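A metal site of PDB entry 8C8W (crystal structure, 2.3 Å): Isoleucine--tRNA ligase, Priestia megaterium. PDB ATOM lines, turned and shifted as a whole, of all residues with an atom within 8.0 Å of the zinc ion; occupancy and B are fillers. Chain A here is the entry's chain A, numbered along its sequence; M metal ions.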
ATOM      1  N   GLU A 458       8.126   1.498  11.200  1.00  0.00           N
ATOM      2  CA  GLU A 458       9.109   2.214  10.398  1.00  0.00           C
ATOM      3  C   GLU A 458       9.557   1.332   9.236  1.00  0.00           C
ATOM      4  O   GLU A 458       9.850   0.149   9.416  1.00  0.00           O
ATOM      5  CB  GLU A 458      10.325   2.616  11.227  1.00  0.00           C
ATOM      6  CG  GLU A 458      10.055   3.715  12.231  1.00  0.00           C
ATOM      7  CD  GLU A 458      11.231   3.933  13.162  1.00  0.00           C
ATOM      8  OE1 GLU A 458      11.417   3.117  14.094  1.00  0.00           O
ATOM      9  OE2 GLU A 458      11.976   4.908  12.950  1.00  0.00           O
ATOM     10  N   CYS A 459       9.613   1.923   8.052  1.00  0.00           N
ATOM     11  CA  CYS A 459      10.090   1.195   6.882  1.00  0.00           C
ATOM     12  C   CYS A 459      11.596   0.989   6.986  1.00  0.00           C
ATOM     13  O   CYS A 459      12.354   1.947   7.212  1.00  0.00           O
ATOM     14  CB  CYS A 459       9.736   1.961   5.608  1.00  0.00           C
ATOM     15  SG  CYS A 459      10.485   1.251   4.133  1.00  0.00           S
ATOM     16  N   GLU A 460      12.037  -0.264   6.805  1.00  0.00           N
ATOM     17  CA  GLU A 460      13.467  -0.560   6.807  1.00  0.00           C
ATOM     18  C   GLU A 460      14.185   0.140   5.665  1.00  0.00           C
ATOM     19  O   GLU A 460      15.371   0.472   5.780  1.00  0.00           O
ATOM     20  CB  GLU A 460      13.688  -2.073   6.729  1.00  0.00           C
ATOM     21  CG  GLU A 460      13.212  -2.856   7.942  1.00  0.00           C
ATOM     22  CD  GLU A 460      14.225  -2.840   9.078  1.00  0.00           C
ATOM     23  OE1 GLU A 460      15.314  -3.438   8.906  1.00  0.00           O
ATOM     24  OE2 GLU A 460      13.929  -2.248  10.140  1.00  0.00           O
ATOM     25  N   GLY A 461      13.488   0.378   4.550  1.00  0.00           N
ATOM     26  CA  GLY A 461      14.106   0.989   3.387  1.00  0.00           C
ATOM     27  C   GLY A 461      14.270   2.487   3.481  1.00  0.00           C
ATOM     28  O   GLY A 461      15.385   2.996   3.323  1.00  0.00           O
ATOM     29  N   CYS A 462      13.182   3.209   3.755  1.00  0.00           N
ATOM     30  CA  CYS A 462      13.177   4.669   3.697  1.00  0.00           C
ATOM     31  C   CYS A 462      12.744   5.334   4.992  1.00  0.00           C
ATOM     32  O   CYS A 462      12.538   6.554   5.012  1.00  0.00           O
ATOM     33  CB  CYS A 462      12.279   5.156   2.565  1.00  0.00           C
ATOM     34  SG  CYS A 462      10.529   4.884   2.869  1.00  0.00           S
ATOM     35  N   GLN A 463      12.580   4.576   6.080  1.00  0.00           N
ATOM     36  CA  GLN A 463      12.293   5.110   7.418  1.00  0.00           C
ATOM     37  C   GLN A 463      10.948   5.834   7.493  1.00  0.00           C
ATOM     38  O   GLN A 463      10.692   6.557   8.462  1.00  0.00           O
ATOM     39  CB  GLN A 463      13.413   6.031   7.903  1.00  0.00           C
ATOM     40  CG  GLN A 463      14.693   5.303   8.273  1.00  0.00           C
ATOM     41  CD  GLN A 463      15.413   4.729   7.067  1.00  0.00           C
ATOM     42  OE1 GLN A 463      15.974   5.467   6.248  1.00  0.00           O
ATOM     43  NE2 GLN A 463      15.401   3.401   6.949  1.00  0.00           N
ATOM     44  N   HIS A 464      10.100   5.671   6.487  1.00  0.00           N
ATOM     45  CA  HIS A 464       8.748   6.203   6.563  1.00  0.00           C
ATOM     46  C   HIS A 464       7.998   5.571   7.739  1.00  0.00           C
ATOM     47  O   HIS A 464       8.206   4.403   8.072  1.00  0.00           O
ATOM     48  CB  HIS A 464       8.000   5.940   5.255  1.00  0.00           C
ATOM     49  CG  HIS A 464       6.581   6.421   5.247  1.00  0.00           C
ATOM     50  ND1 HIS A 464       6.253   7.748   5.098  1.00  0.00           N
ATOM     51  CD2 HIS A 464       5.414   5.757   5.377  1.00  0.00           C
ATOM     52  CE1 HIS A 464       4.940   7.883   5.132  1.00  0.00           C
ATOM     53  NE2 HIS A 464       4.400   6.690   5.294  1.00  0.00           N
ATOM     54  N   GLN A 465       7.145   6.355   8.382  1.00  0.00           N
ATOM     55  CA  GLN A 465       6.452   5.935   9.593  1.00  0.00           C
ATOM     56  C   GLN A 465       4.960   5.793   9.322  1.00  0.00           C
ATOM     57  O   GLN A 465       4.356   6.644   8.666  1.00  0.00           O
ATOM     58  CB  GLN A 465       6.686   6.919  10.736  1.00  0.00           C
ATOM     59  CG  GLN A 465       8.149   7.043  11.140  1.00  0.00           C
ATOM     60  CD  GLN A 465       8.375   8.077  12.221  1.00  0.00           C
ATOM     61  OE1 GLN A 465       7.425   8.603  12.809  1.00  0.00           O
ATOM     62  NE2 GLN A 465       9.634   8.385  12.490  1.00  0.00           N
ATOM     63  N   LEU A 498       4.380  -4.424   7.915  1.00  0.00           N
ATOM     64  CA  LEU A 498       3.566  -3.665   6.980  1.00  0.00           C
ATOM     65  C   LEU A 498       4.363  -3.394   5.712  1.00  0.00           C
ATOM     66  O   LEU A 498       5.595  -3.290   5.740  1.00  0.00           O
ATOM     67  CB  LEU A 498       3.105  -2.335   7.588  1.00  0.00           C
ATOM     68  CG  LEU A 498       2.545  -2.338   9.016  1.00  0.00           C
ATOM     69  CD1 LEU A 498       2.105  -0.952   9.409  1.00  0.00           C
ATOM     70  CD2 LEU A 498       1.407  -3.324   9.167  1.00  0.00           C
ATOM     71  N   THR A 499       3.647  -3.277   4.592  1.00  0.00           N
ATOM     72  CA  THR A 499       4.260  -2.878   3.336  1.00  0.00           C
ATOM     73  C   THR A 499       4.288  -1.358   3.257  1.00  0.00           C
ATOM     74  O   THR A 499       3.265  -0.696   3.448  1.00  0.00           O
ATOM     75  CB  THR A 499       3.478  -3.461   2.148  1.00  0.00           C
ATOM     76  OG1 THR A 499       3.366  -4.882   2.304  1.00  0.00           O
ATOM     77  CG2 THR A 499       4.203  -3.167   0.844  1.00  0.00           C
ATOM     78  N   CYS A 500       5.469  -0.803   2.986  1.00  0.00           N
ATOM     79  CA  CYS A 500       5.626   0.646   2.989  1.00  0.00           C
ATOM     80  C   CYS A 500       4.787   1.257   1.872  1.00  0.00           C
ATOM     81  O   CYS A 500       4.876   0.807   0.719  1.00  0.00           O
ATOM     82  CB  CYS A 500       7.086   1.030   2.815  1.00  0.00           C
ATOM     83  SG  CYS A 500       7.358   2.825   2.773  1.00  0.00           S
ATOM     84  N   PRO A 501       3.966   2.270   2.153  1.00  0.00           N
ATOM     85  CA  PRO A 501       3.206   2.932   1.080  1.00  0.00           C
ATOM     86  C   PRO A 501       4.083   3.734   0.129  1.00  0.00           C
ATOM     87  O   PRO A 501       3.614   4.098  -0.952  1.00  0.00           O
ATOM     88  CB  PRO A 501       2.238   3.836   1.835  1.00  0.00           C
ATOM     89  CG  PRO A 501       2.905   4.094   3.149  1.00  0.00           C
ATOM     90  CD  PRO A 501       3.653   2.838   3.483  1.00  0.00           C
ATOM     91  N   VAL A 502       5.331   4.012   0.491  1.00  0.00           N
ATOM     92  CA  VAL A 502       6.203   4.840  -0.322  1.00  0.00           C
ATOM     93  C   VAL A 502       7.051   3.973  -1.251  1.00  0.00           C
ATOM     94  O   VAL A 502       7.018   4.148  -2.477  1.00  0.00           O
ATOM     95  CB  VAL A 502       7.109   5.736   0.559  1.00  0.00           C
ATOM     96  CG1 VAL A 502       8.196   6.384  -0.285  1.00  0.00           C
ATOM     97  CG2 VAL A 502       6.270   6.772   1.276  1.00  0.00           C
ATOM     98  N   CYS A 503       7.808   3.048  -0.676  1.00  0.00           N
ATOM     99  CA  CYS A 503       8.743   2.238  -1.442  1.00  0.00           C
ATOM    100  C   CYS A 503       8.429   0.749  -1.431  1.00  0.00           C
ATOM    101  O   CYS A 503       9.210  -0.038  -1.976  1.00  0.00           O
ATOM    102  CB  CYS A 503      10.171   2.458  -0.917  1.00  0.00           C
ATOM    103  SG  CYS A 503      10.481   1.630   0.661  1.00  0.00           S
ATOM    104  N   SER A 504       7.312   0.336  -0.819  1.00  0.00           N
ATOM    105  CA  SER A 504       6.917  -1.067  -0.715  1.00  0.00           C
ATOM    106  C   SER A 504       7.947  -1.902   0.040  1.00  0.00           C
ATOM    107  O   SER A 504       7.968  -3.130  -0.092  1.00  0.00           O
ATOM    108  CB  SER A 504       6.629  -1.677  -2.092  1.00  0.00           C
ATOM    109  OG  SER A 504       6.057  -2.969  -1.967  1.00  0.00           O
ATOM    110  N   GLY A 505       8.800  -1.270   0.843  1.00  0.00           N
ATOM    111  CA  GLY A 505       9.718  -1.985   1.697  1.00  0.00           C
ATOM    112  C   GLY A 505       9.018  -2.556   2.916  1.00  0.00           C
ATOM    113  O   GLY A 505       7.813  -2.375   3.142  1.00  0.00           O
ATOM    114  N   GLU A 506       9.783  -3.286   3.727  1.00  0.00           N
ATOM    115  CA  GLU A 506       9.256  -3.879   4.944  1.00  0.00           C
ATOM    116  C   GLU A 506       9.211  -2.826   6.051  1.00  0.00           C
ATOM    117  O   GLU A 506      10.193  -2.115   6.293  1.00  0.00           O
ATOM    118  CB  GLU A 506      10.122  -5.057   5.378  1.00  0.00           C
ATOM    119  CG  GLU A 506       9.557  -5.864   6.543  1.00  0.00           C
ATOM    120  CD  GLU A 506      10.521  -6.915   7.054  1.00  0.00           C
ATOM    121  OE1 GLU A 506      11.742  -6.766   6.836  1.00  0.00           O
ATOM    122  OE2 GLU A 506      10.065  -7.892   7.680  1.00  0.00           O
ATOM    123  N   MET A 507       8.069  -2.716   6.715  1.00  0.00           N
ATOM    124  CA  MET A 507       7.914  -1.840   7.872  1.00  0.00           C
ATOM    125  C   MET A 507       7.853  -2.690   9.131  1.00  0.00           C
ATOM    126  O   MET A 507       7.053  -3.634   9.194  1.00  0.00           O
ATOM    127  CB  MET A 507       6.663  -0.973   7.767  1.00  0.00           C
ATOM    128  CG  MET A 507       6.544  -0.162   6.486  1.00  0.00           C
ATOM    129  SD  MET A 507       5.181   1.033   6.557  1.00  0.00           S
ATOM    130  CE  MET A 507       5.967   2.362   7.457  1.00  0.00           C
HETATM  131 ZN    ZN M   1       9.665   2.747   2.553  1.00  0.00          ZN
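The zinc ion is bound by SG of Cys 500 (2.3 Å), SG of Cys 459 (2.3 Å), SG of Cys 462 (2.3 Å) and SG of Cys 503 (2.3 Å).
The side-chain sulfur of Cys 500 lies close to the backbone NH of Val 502. The backbone carbonyl oxygen (O) of Gly 505 is in hydrogen-bond range of the backbone NH (N) of Cys 500, at 2.8 Å. N of Cys 459 is in hydrogen-bond range of O of His 464 (2.9 Å). SG of Cys 459 sits close to N of Gly 461 (3.2 Å). NE2 of Gln 463 sits close to O of Cys 459 (3.4 Å). N of His 464 lies close to SG of Cys 462, at 3.7 Å. The backbone NH of Gly 505 lies close to the side-chain sulfur of Cys 503 (3.4 Å).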
